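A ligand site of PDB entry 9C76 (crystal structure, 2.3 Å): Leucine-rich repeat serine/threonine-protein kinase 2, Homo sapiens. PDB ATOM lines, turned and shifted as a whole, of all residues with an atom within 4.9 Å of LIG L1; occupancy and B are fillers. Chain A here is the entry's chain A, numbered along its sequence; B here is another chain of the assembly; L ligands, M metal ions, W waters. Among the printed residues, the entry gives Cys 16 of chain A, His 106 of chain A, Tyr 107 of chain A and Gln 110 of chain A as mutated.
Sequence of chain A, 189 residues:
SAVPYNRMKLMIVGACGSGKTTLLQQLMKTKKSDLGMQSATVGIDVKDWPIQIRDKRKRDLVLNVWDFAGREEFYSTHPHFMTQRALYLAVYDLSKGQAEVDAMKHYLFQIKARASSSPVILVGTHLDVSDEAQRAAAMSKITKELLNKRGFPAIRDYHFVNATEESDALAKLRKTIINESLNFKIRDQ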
ATOM      1  N   MET A  11       7.025  14.668   4.462  1.00  0.00           N
ATOM      2  CA  MET A  11       7.996  15.376   5.286  1.00  0.00           C
ATOM      3  C   MET A  11       7.423  16.733   5.646  1.00  0.00           C
ATOM      4  O   MET A  11       7.169  17.556   4.752  1.00  0.00           O
ATOM      5  CB  MET A  11       9.326  15.501   4.539  1.00  0.00           C
ATOM      6  CG  MET A  11       9.989  14.163   4.294  1.00  0.00           C
ATOM      7  SD  MET A  11      11.043  13.656   5.669  1.00  0.00           S
ATOM      8  CE  MET A  11      12.470  14.658   5.343  1.00  0.00           C
ATOM      9  N   VAL A  13       8.156  20.171   7.303  1.00  0.00           N
ATOM     10  CA  VAL A  13       9.283  21.014   7.659  1.00  0.00           C
ATOM     11  C   VAL A  13       8.770  22.418   7.958  1.00  0.00           C
ATOM     12  O   VAL A  13       7.631  22.771   7.623  1.00  0.00           O
ATOM     13  CB  VAL A  13      10.333  21.082   6.512  1.00  0.00           C
ATOM     14  CG1 VAL A  13      10.685  19.696   6.044  1.00  0.00           C
ATOM     15  CG2 VAL A  13       9.824  21.952   5.367  1.00  0.00           C
ATOM     16  N   GLY A  14       9.604  23.227   8.598  1.00  0.00           N
ATOM     17  CA  GLY A  14       9.275  24.617   8.890  1.00  0.00           C
ATOM     18  C   GLY A  14       9.903  25.015  10.209  1.00  0.00           C
ATOM     19  O   GLY A  14      10.351  24.216  11.016  1.00  0.00           O
ATOM     20  N   CYS A  16      10.573  26.327  13.994  1.00  0.00           N
ATOM     21  CA  CYS A  16      10.006  25.860  15.246  1.00  0.00           C
ATOM     22  C   CYS A  16       8.846  26.763  15.648  1.00  0.00           C
ATOM     23  O   CYS A  16       8.920  27.986  15.524  1.00  0.00           O
ATOM     24  CB  CYS A  16      11.094  25.836  16.328  1.00  0.00           C
ATOM     25  SG  CYS A  16      10.930  24.533  17.595  1.00  0.00           S
ATOM     26  N   GLY A  17       7.766  26.154  16.129  1.00  0.00           N
ATOM     27  CA  GLY A  17       6.587  26.900  16.487  1.00  0.00           C
ATOM     28  C   GLY A  17       5.646  27.248  15.350  1.00  0.00           C
ATOM     29  O   GLY A  17       4.668  27.972  15.573  1.00  0.00           O
ATOM     30  N   LYS A  20       3.478  22.727  13.200  1.00  0.00           N
ATOM     31  CA  LYS A  20       3.589  21.514  12.397  1.00  0.00           C
ATOM     32  C   LYS A  20       2.929  20.330  13.094  1.00  0.00           C
ATOM     33  O   LYS A  20       2.104  19.622  12.489  1.00  0.00           O
ATOM     34  CB  LYS A  20       5.062  21.209  12.102  1.00  0.00           C
ATOM     35  CG  LYS A  20       5.744  22.293  11.259  1.00  0.00           C
ATOM     36  CD  LYS A  20       7.169  21.920  10.859  1.00  0.00           C
ATOM     37  CE  LYS A  20       8.079  21.664  12.066  1.00  0.00           C
ATOM     38  NZ  LYS A  20       8.351  22.900  12.857  1.00  0.00           N
ATOM     39  N   TYR A  88       6.761  17.152   0.489  1.00  0.00           N
ATOM     40  CA  TYR A  88       7.102  18.034   1.602  1.00  0.00           C
ATOM     41  C   TYR A  88       5.938  18.958   1.926  1.00  0.00           C
ATOM     42  O   TYR A  88       5.307  19.516   1.024  1.00  0.00           O
ATOM     43  CB  TYR A  88       8.350  18.849   1.261  1.00  0.00           C
ATOM     44  CG  TYR A  88       9.629  18.043   1.382  1.00  0.00           C
ATOM     45  CD1 TYR A  88       9.989  17.126   0.404  1.00  0.00           C
ATOM     46  CD2 TYR A  88      10.469  18.204   2.471  1.00  0.00           C
ATOM     47  CE1 TYR A  88      11.143  16.382   0.514  1.00  0.00           C
ATOM     48  CE2 TYR A  88      11.626  17.470   2.590  1.00  0.00           C
ATOM     49  CZ  TYR A  88      11.963  16.571   1.609  1.00  0.00           C
ATOM     50  OH  TYR A  88      13.120  15.837   1.728  1.00  0.00           O
ATOM     51  N   HIS A 106      14.647  29.501   3.170  1.00  0.00           N
ATOM     52  CA  HIS A 106      15.831  28.668   3.385  1.00  0.00           C
ATOM     53  C   HIS A 106      15.441  27.181   3.281  1.00  0.00           C
ATOM     54  O   HIS A 106      16.098  26.406   2.578  1.00  0.00           O
ATOM     55  CB  HIS A 106      16.495  29.005   4.719  1.00  0.00           C
ATOM     56  CG  HIS A 106      17.802  28.304   4.932  1.00  0.00           C
ATOM     57  ND1 HIS A 106      18.360  27.459   3.996  1.00  0.00           N
ATOM     58  CD2 HIS A 106      18.677  28.343   5.963  1.00  0.00           C
ATOM     59  CE1 HIS A 106      19.516  26.994   4.444  1.00  0.00           C
ATOM     60  NE2 HIS A 106      19.734  27.525   5.636  1.00  0.00           N
ATOM     61  N   TYR A 107      14.348  26.796   3.938  1.00  0.00           N
ATOM     62  CA  TYR A 107      13.910  25.404   3.828  1.00  0.00           C
ATOM     63  C   TYR A 107      13.718  25.027   2.362  1.00  0.00           C
ATOM     64  O   TYR A 107      14.229  23.992   1.903  1.00  0.00           O
ATOM     65  CB  TYR A 107      12.616  25.158   4.605  1.00  0.00           C
ATOM     66  CG  TYR A 107      12.775  25.090   6.099  1.00  0.00           C
ATOM     67  CD1 TYR A 107      13.153  23.903   6.714  1.00  0.00           C
ATOM     68  CD2 TYR A 107      12.536  26.193   6.913  1.00  0.00           C
ATOM     69  CE1 TYR A 107      13.314  23.816   8.075  1.00  0.00           C
ATOM     70  CE2 TYR A 107      12.678  26.111   8.286  1.00  0.00           C
ATOM     71  CZ  TYR A 107      13.072  24.917   8.860  1.00  0.00           C
ATOM     72  OH  TYR A 107      13.220  24.812  10.224  1.00  0.00           O
ATOM     73  N   GLN A 110      16.967  24.267   0.805  1.00  0.00           N
ATOM     74  CA  GLN A 110      17.390  22.936   1.210  1.00  0.00           C
ATOM     75  C   GLN A 110      16.652  21.891   0.394  1.00  0.00           C
ATOM     76  O   GLN A 110      17.265  21.087  -0.307  1.00  0.00           O
ATOM     77  CB  GLN A 110      17.130  22.735   2.709  1.00  0.00           C
ATOM     78  CG  GLN A 110      17.370  21.320   3.255  1.00  0.00           C
ATOM     79  CD  GLN A 110      18.848  20.985   3.444  1.00  0.00           C
ATOM     80  OE1 GLN A 110      19.641  21.837   3.783  1.00  0.00           O
ATOM     81  NE2 GLN A 110      19.182  19.730   3.337  1.00  0.00           N
ATOM     82  N   ILE A 111      15.328  21.975   0.382  1.00  0.00           N
ATOM     83  CA  ILE A 111      14.553  20.935  -0.273  1.00  0.00           C
ATOM     84  C   ILE A 111      14.842  20.960  -1.766  1.00  0.00           C
ATOM     85  O   ILE A 111      14.914  19.911  -2.427  1.00  0.00           O
ATOM     86  CB  ILE A 111      13.069  21.106   0.026  1.00  0.00           C
ATOM     87  CG1 ILE A 111      12.840  21.247   1.529  1.00  0.00           C
ATOM     88  CG2 ILE A 111      12.306  19.858  -0.404  1.00  0.00           C
ATOM     89  CD1 ILE A 111      11.514  21.880   1.887  1.00  0.00           C
ATOM     90  N   ARG A 114      18.411  19.292  -2.075  1.00  0.00           N
ATOM     91  CA  ARG A 114      18.501  17.938  -1.576  1.00  0.00           C
ATOM     92  C   ARG A 114      17.546  16.981  -2.274  1.00  0.00           C
ATOM     93  O   ARG A 114      17.781  15.765  -2.252  1.00  0.00           O
ATOM     94  CB  ARG A 114      18.141  17.950  -0.094  1.00  0.00           C
ATOM     95  CG  ARG A 114      18.873  18.965   0.680  1.00  0.00           C
ATOM     96  CD  ARG A 114      20.285  18.478   0.933  1.00  0.00           C
ATOM     97  NE  ARG A 114      20.225  17.329   1.824  1.00  0.00           N
ATOM     98  CZ  ARG A 114      21.251  16.537   2.105  1.00  0.00           C
ATOM     99  NH1 ARG A 114      22.435  16.740   1.555  1.00  0.00           N
ATOM    100  NH2 ARG A 114      21.093  15.535   2.957  1.00  0.00           N
ATOM    101  N   PHE B  68       9.551  16.594  12.917  1.00  0.00           N
ATOM    102  CA  PHE B  68      10.874  16.809  13.488  1.00  0.00           C
ATOM    103  C   PHE B  68      10.812  17.765  14.671  1.00  0.00           C
ATOM    104  O   PHE B  68      10.064  18.746  14.660  1.00  0.00           O
ATOM    105  CB  PHE B  68      11.834  17.361  12.437  1.00  0.00           C
ATOM    106  CG  PHE B  68      12.104  16.407  11.298  1.00  0.00           C
ATOM    107  CD1 PHE B  68      11.283  16.394  10.187  1.00  0.00           C
ATOM    108  CD2 PHE B  68      13.176  15.531  11.353  1.00  0.00           C
ATOM    109  CE1 PHE B  68      11.530  15.528   9.140  1.00  0.00           C
ATOM    110  CE2 PHE B  68      13.418  14.653  10.311  1.00  0.00           C
ATOM    111  CZ  PHE B  68      12.597  14.658   9.202  1.00  0.00           C
ATOM    112  N   ALA B  69      11.604  17.469  15.696  1.00  0.00           N
ATOM    113  CA  ALA B  69      11.758  18.280  16.893  1.00  0.00           C
ATOM    114  C   ALA B  69      13.248  18.488  17.156  1.00  0.00           C
ATOM    115  O   ALA B  69      14.110  17.909  16.482  1.00  0.00           O
ATOM    116  CB  ALA B  69      11.094  17.621  18.109  1.00  0.00           C
ATOM    117  N   GLY B  70      13.557  19.238  18.210  1.00  0.00           N
ATOM    118  CA  GLY B  70      14.939  19.480  18.600  1.00  0.00           C
ATOM    119  C   GLY B  70      15.375  20.904  18.299  1.00  0.00           C
ATOM    120  O   GLY B  70      14.593  21.752  17.858  1.00  0.00           O
ATOM    121  N   ARG B  71      16.644  21.162  18.573  1.00  0.00           N
ATOM    122  CA  ARG B  71      17.226  22.482  18.392  1.00  0.00           C
ATOM    123  C   ARG B  71      17.733  22.670  16.964  1.00  0.00           C
ATOM    124  O   ARG B  71      18.209  21.734  16.313  1.00  0.00           O
ATOM    125  CB  ARG B  71      18.381  22.695  19.378  1.00  0.00           C
ATOM    126  N   GLU B  72      17.606  23.906  16.480  1.00  0.00           N
ATOM    127  CA  GLU B  72      18.019  24.228  15.113  1.00  0.00           C
ATOM    128  C   GLU B  72      19.515  24.015  14.913  1.00  0.00           C
ATOM    129  O   GLU B  72      19.966  23.689  13.798  1.00  0.00           O
ATOM    130  CB  GLU B  72      17.654  25.683  14.823  1.00  0.00           C
ATOM    131  CG  GLU B  72      17.634  26.082  13.368  1.00  0.00           C
ATOM    132  CD  GLU B  72      17.167  27.515  13.178  1.00  0.00           C
ATOM    133  OE1 GLU B  72      16.394  28.014  14.027  1.00  0.00           O
ATOM    134  OE2 GLU B  72      17.588  28.163  12.193  1.00  0.00           O
ATOM    135  N   TYR B  75      20.474  20.627  13.354  1.00  0.00           N
ATOM    136  CA  TYR B  75      20.218  20.473  11.937  1.00  0.00           C
ATOM    137  C   TYR B  75      21.196  21.305  11.120  1.00  0.00           C
ATOM    138  O   TYR B  75      21.521  20.937   9.981  1.00  0.00           O
ATOM    139  CB  TYR B  75      18.778  20.847  11.615  1.00  0.00           C
ATOM    140  CG  TYR B  75      17.771  19.916  12.248  1.00  0.00           C
ATOM    141  CD1 TYR B  75      17.344  18.766  11.579  1.00  0.00           C
ATOM    142  CD2 TYR B  75      17.260  20.155  13.514  1.00  0.00           C
ATOM    143  CE1 TYR B  75      16.440  17.893  12.146  1.00  0.00           C
ATOM    144  CE2 TYR B  75      16.354  19.281  14.095  1.00  0.00           C
ATOM    145  CZ  TYR B  75      15.941  18.157  13.403  1.00  0.00           C
ATOM    146  OH  TYR B  75      15.046  17.289  13.972  1.00  0.00           O
ATOM    147  N   HIS B  78      24.435  19.037  11.238  1.00  0.00           N
ATOM    148  CA  HIS B  78      24.304  17.702  10.661  1.00  0.00           C
ATOM    149  C   HIS B  78      23.568  17.801   9.341  1.00  0.00           C
ATOM    150  O   HIS B  78      22.406  17.389   9.224  1.00  0.00           O
ATOM    151  CB  HIS B  78      23.557  16.789  11.633  1.00  0.00           C
ATOM    152  CG  HIS B  78      24.267  16.554  12.932  1.00  0.00           C
ATOM    153  ND1 HIS B  78      24.221  17.451  13.981  1.00  0.00           N
ATOM    154  CD2 HIS B  78      24.978  15.490  13.391  1.00  0.00           C
ATOM    155  CE1 HIS B  78      24.924  16.977  14.995  1.00  0.00           C
ATOM    156  NE2 HIS B  78      25.380  15.781  14.673  1.00  0.00           N
ATOM    157  N   PRO B  79      24.232  18.312   8.296  1.00  0.00           N
ATOM    158  CA  PRO B  79      23.525  18.549   7.028  1.00  0.00           C
ATOM    159  C   PRO B  79      23.000  17.292   6.348  1.00  0.00           C
ATOM    160  O   PRO B  79      21.992  17.367   5.645  1.00  0.00           O
ATOM    161  CB  PRO B  79      24.584  19.247   6.153  1.00  0.00           C
ATOM    162  CG  PRO B  79      25.917  18.927   6.808  1.00  0.00           C
ATOM    163  CD  PRO B  79      25.616  18.817   8.281  1.00  0.00           C
ATOM    164  N   HIS B  80      23.665  16.141   6.526  1.00  0.00           N
ATOM    165  CA  HIS B  80      23.272  14.911   5.841  1.00  0.00           C
ATOM    166  C   HIS B  80      22.835  13.838   6.837  1.00  0.00           C
ATOM    167  O   HIS B  80      23.015  12.638   6.581  1.00  0.00           O
ATOM    168  CB  HIS B  80      24.405  14.362   4.973  1.00  0.00           C
ATOM    169  CG  HIS B  80      24.963  15.354   3.999  1.00  0.00           C
ATOM    170  ND1 HIS B  80      24.872  15.191   2.630  1.00  0.00           N
ATOM    171  CD2 HIS B  80      25.663  16.505   4.186  1.00  0.00           C
ATOM    172  CE1 HIS B  80      25.461  16.202   2.022  1.00  0.00           C
ATOM    173  NE2 HIS B  80      25.942  17.012   2.945  1.00  0.00           N
ATOM    174  N   PHE B  81      22.238  14.229   7.966  1.00  0.00           N
ATOM    175  CA  PHE B  81      22.008  13.260   9.032  1.00  0.00           C
ATOM    176  C   PHE B  81      20.947  12.223   8.681  1.00  0.00           C
ATOM    177  O   PHE B  81      20.835  11.215   9.382  1.00  0.00           O
ATOM    178  CB  PHE B  81      21.635  13.980  10.341  1.00  0.00           C
ATOM    179  CG  PHE B  81      20.171  14.289  10.508  1.00  0.00           C
ATOM    180  CD1 PHE B  81      19.567  15.352   9.852  1.00  0.00           C
ATOM    181  CD2 PHE B  81      19.408  13.524  11.371  1.00  0.00           C
ATOM    182  CE1 PHE B  81      18.215  15.616  10.037  1.00  0.00           C
ATOM    183  CE2 PHE B  81      18.066  13.786  11.565  1.00  0.00           C
ATOM    184  CZ  PHE B  81      17.467  14.827  10.901  1.00  0.00           C
ATOM    185  N   MET B  82      20.183  12.410   7.598  1.00  0.00           N
ATOM    186  CA  MET B  82      19.171  11.438   7.178  1.00  0.00           C
ATOM    187  C   MET B  82      19.622  10.552   6.026  1.00  0.00           C
ATOM    188  O   MET B  82      18.803   9.782   5.502  1.00  0.00           O
ATOM    189  CB  MET B  82      17.864  12.145   6.828  1.00  0.00           C
ATOM    190  CG  MET B  82      17.223  12.771   8.041  1.00  0.00           C
ATOM    191  SD  MET B  82      15.577  13.341   7.764  1.00  0.00           S
ATOM    192  CE  MET B  82      15.817  14.498   6.445  1.00  0.00           C
HETATM  193  N1  LIG L   1      19.292  17.047   6.672  1.00  0.00           N
HETATM  194  C1  LIG L   1      16.413  19.045   7.084  1.00  0.00           C
HETATM  195  C2  LIG L   1      15.982  19.885   8.227  1.00  0.00           C
HETATM  196  C3  LIG L   1      15.024  19.476   9.157  1.00  0.00           C
HETATM  197  C4  LIG L   1      14.669  20.279  10.210  1.00  0.00           C
HETATM  198  C5  LIG L   1      15.283  21.543  10.393  1.00  0.00           C
HETATM  199  C6  LIG L   1      11.890  21.042  12.919  1.00  0.00           C
HETATM  200  C7  LIG L   1      13.509  21.237  14.698  1.00  0.00           C
HETATM  201  C8  LIG L   1      16.617  25.645   6.356  1.00  0.00           C
HETATM  202  C9  LIG L   1      16.290  26.605   7.506  1.00  0.00           C
HETATM  203  C10 LIG L   1      16.627  21.102   8.411  1.00  0.00           C
HETATM  204  C11 LIG L   1      15.735  18.922   5.859  1.00  0.00           C
HETATM  205  C12 LIG L   1      14.434  19.609   5.574  1.00  0.00           C
HETATM  206  N2  LIG L   1      16.923  23.142   9.622  1.00  0.00           N
HETATM  207  C13 LIG L   1      16.575  23.907  10.651  1.00  0.00           C
HETATM  208  N3  LIG L   1      15.644  23.616  11.556  1.00  0.00           N
HETATM  209  C14 LIG L   1      15.018  22.439  11.476  1.00  0.00           C
HETATM  210  N4  LIG L   1      14.039  22.194  12.442  1.00  0.00           N
HETATM  211  C15 LIG L   1      12.650  21.982  12.011  1.00  0.00           C
HETATM  212  C16 LIG L   1      16.291  21.943   9.480  1.00  0.00           C
HETATM  213  N5  LIG L   1      17.584  18.425   7.321  1.00  0.00           N
HETATM  214  C17 LIG L   1      18.131  17.640   6.375  1.00  0.00           C
HETATM  215  O1  LIG L   1       9.956  21.298  14.974  1.00  0.00           O
HETATM  216  O2  LIG L   1      17.207  25.079  10.725  1.00  0.00           O
HETATM  217  C18 LIG L   1      14.143  23.723  14.302  1.00  0.00           C
HETATM  218  N6  LIG L   1      12.101  21.361  14.324  1.00  0.00           N
HETATM  219  C19 LIG L   1      11.114  21.609  15.209  1.00  0.00           C
HETATM  220  N7  LIG L   1      17.790  24.897   8.214  1.00  0.00           N
HETATM  221  C20 LIG L   1      11.491  22.273  16.530  1.00  0.00           C
HETATM  222  C21 LIG L   1      17.282  26.205   8.633  1.00  0.00           C
HETATM  223  C22 LIG L   1      16.623  26.162   9.996  1.00  0.00           C
HETATM  224  C23 LIG L   1      10.312  22.888  17.148  1.00  0.00           C
HETATM  225  C24 LIG L   1      14.311  22.259  13.925  1.00  0.00           C
HETATM  226  C25 LIG L   1      16.935  24.380   7.146  1.00  0.00           C
HETATM  227  C26 LIG L   1      16.298  18.095   4.868  1.00  0.00           C
HETATM  228  C27 LIG L   1      15.618  17.909   3.541  1.00  0.00           C
HETATM  229  C28 LIG L   1      17.501  17.454   5.131  1.00  0.00           C
HETATM  230  C29 LIG L   1      19.190  24.973   7.810  1.00  0.00           C
HETATM  231 CL1  LIG L   1      14.235  17.951   8.943  1.00  0.00          CL
HETATM  232  F1  LIG L   1      17.579  21.500   7.530  1.00  0.00           F
HETATM  233  F2  LIG L   1      14.449  20.316   4.446  1.00  0.00           F
HETATM  234  F3  LIG L   1      14.034  20.464   6.493  1.00  0.00           F
HETATM  235  F4  LIG L   1      13.438  18.754   5.432  1.00  0.00           F
HETATM  236  P1  LG2 L   2       5.920  23.080  15.614  1.00  0.00           P
HETATM  237  O1  LG2 L   2       5.523  21.645  15.376  1.00  0.00           O
HETATM  238  O2  LG2 L   2       7.125  23.190  16.540  1.00  0.00           O
HETATM  239  O3  LG2 L   2       6.091  23.888  14.356  1.00  0.00           O
HETATM  240  O4  LG2 L   2       4.691  23.735  16.445  1.00  0.00           O
HETATM  241  P2  LG2 L   2       3.737  23.077  17.550  1.00  0.00           P
HETATM  242  O5  LG2 L   2       2.551  22.477  16.875  1.00  0.00           O
HETATM  243  O6  LG2 L   2       4.564  22.148  18.369  1.00  0.00           O
HETATM  244  O7  LG2 L   2       3.296  24.312  18.461  1.00  0.00           O
HETATM  245  C1  LG2 L   2       2.674  25.422  17.800  1.00  0.00           C
HETATM  246  C2  LG2 L   2       1.883  26.208  18.819  1.00  0.00           C
HETATM  247  O8  LG2 L   2       1.039  27.137  18.105  1.00  0.00           O
HETATM  248  C3  LG2 L   2       0.936  25.364  19.685  1.00  0.00           C
HETATM  249  O9  LG2 L   2       0.624  26.013  20.903  1.00  0.00           O
HETATM  250  C4  LG2 L   2      -0.277  25.249  18.756  1.00  0.00           C
HETATM  251  O10 LG2 L   2      -1.491  24.970  19.415  1.00  0.00           O
HETATM  252  C5  LG2 L   2      -0.303  26.669  18.184  1.00  0.00           C
HETATM  253  N1  LG2 L   2      -0.863  26.739  16.832  1.00  0.00           N
HETATM  254  C6  LG2 L   2      -0.504  25.980  15.748  1.00  0.00           C
HETATM  255  N2  LG2 L   2      -1.169  26.265  14.654  1.00  0.00           N
HETATM  256  C7  LG2 L   2      -2.039  27.275  15.042  1.00  0.00           C
HETATM  257  C8  LG2 L   2      -3.010  27.984  14.290  1.00  0.00           C
HETATM  258  O11 LG2 L   2      -3.305  27.850  13.093  1.00  0.00           O
HETATM  259  N3  LG2 L   2      -3.666  28.931  15.072  1.00  0.00           N
HETATM  260  C9  LG2 L   2      -3.418  29.171  16.403  1.00  0.00           C
HETATM  261  N4  LG2 L   2      -4.160  30.125  16.993  1.00  0.00           N
HETATM  262  N5  LG2 L   2      -2.507  28.515  17.112  1.00  0.00           N
HETATM  263  C10 LG2 L   2      -1.859  27.581  16.374  1.00  0.00           C
HETATM  264 MG    MG M   1       6.481  19.563  17.374  1.00  0.00          MG
HETATM  265  O   HOH W   1      19.080  28.865   9.970  1.00  0.00           O
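SG of Cys 16 is covalently linked to C23 of LIG L1, 1.8 Å away.
The backbone carbonyl oxygen of Phe 68 of chain B lies close to an oxygen (O1) of LIG L1, at 2.6 Å.
The backbone carbonyl oxygen (O) of Pro 79 of chain B sits at hydrogen-bond distance from a nitrogen (N1) of LIG L1 (2.9 Å).
OH of Tyr 107 sits at hydrogen-bond distance from N3 of LIG L1.
O1 of LIG L1 sits at hydrogen-bond distance from NZ of Lys 20.
O3 of LG2 L2 sits at hydrogen-bond distance from N of Lys 20, at 3.1 Å.
O3 of LG2 L2 lies within salt-bridge range of NZ of Lys 20, at 2.9 Å.
The backbone NH of Gly 17 sits at hydrogen-bond distance from an oxygen (O2) of LG2 L2, at 3.1 Å.
The guanidinium group of Arg 114 sits at hydrogen-bond distance from the backbone carbonyl oxygen of Pro 79 of chain B.
OH of Tyr 107 lies within hydrogen-bond range of O of Gly 14 (3.0 Å).
O of Gly 14 sits at hydrogen-bond distance from NZ of Lys 20.
NE of Arg 114 lies close to NE2 of Gln 110, 3.0 Å away.
The backbone carbonyl oxygen of Ala 69 of chain B lies within hydrogen-bond range of the side-chain hydroxyl of Tyr 75 of chain B, at 2.7 Å.
An oxygen (O2) of LIG L1 lies close to the side-chain carboxylate of Glu 72 of chain B.
Residues that only touch LIG L1: Val 13, His 106, Gln 110, Gly 14, Tyr 75 of chain B, Gly 70 of chain B, Ile 111, Tyr 88, Phe 81 of chain B, Met 82 of chain B and Ala 69 of chain B.
Hydrophobic or aromatic side chains within 4 Å of LIG L1: Val 13, Tyr 88, His 106, Tyr 107, Ile 111, Phe 68 of chain B, Tyr 75 of chain B, Phe 81 of chain B and Met 82 of chain B.
Along chain A the residues within 4 Å of LIG L1 span positions 13 to 111.
The nearest printed residue that does not touch LIG L1 is His 78 of chain B (4.04 Å).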
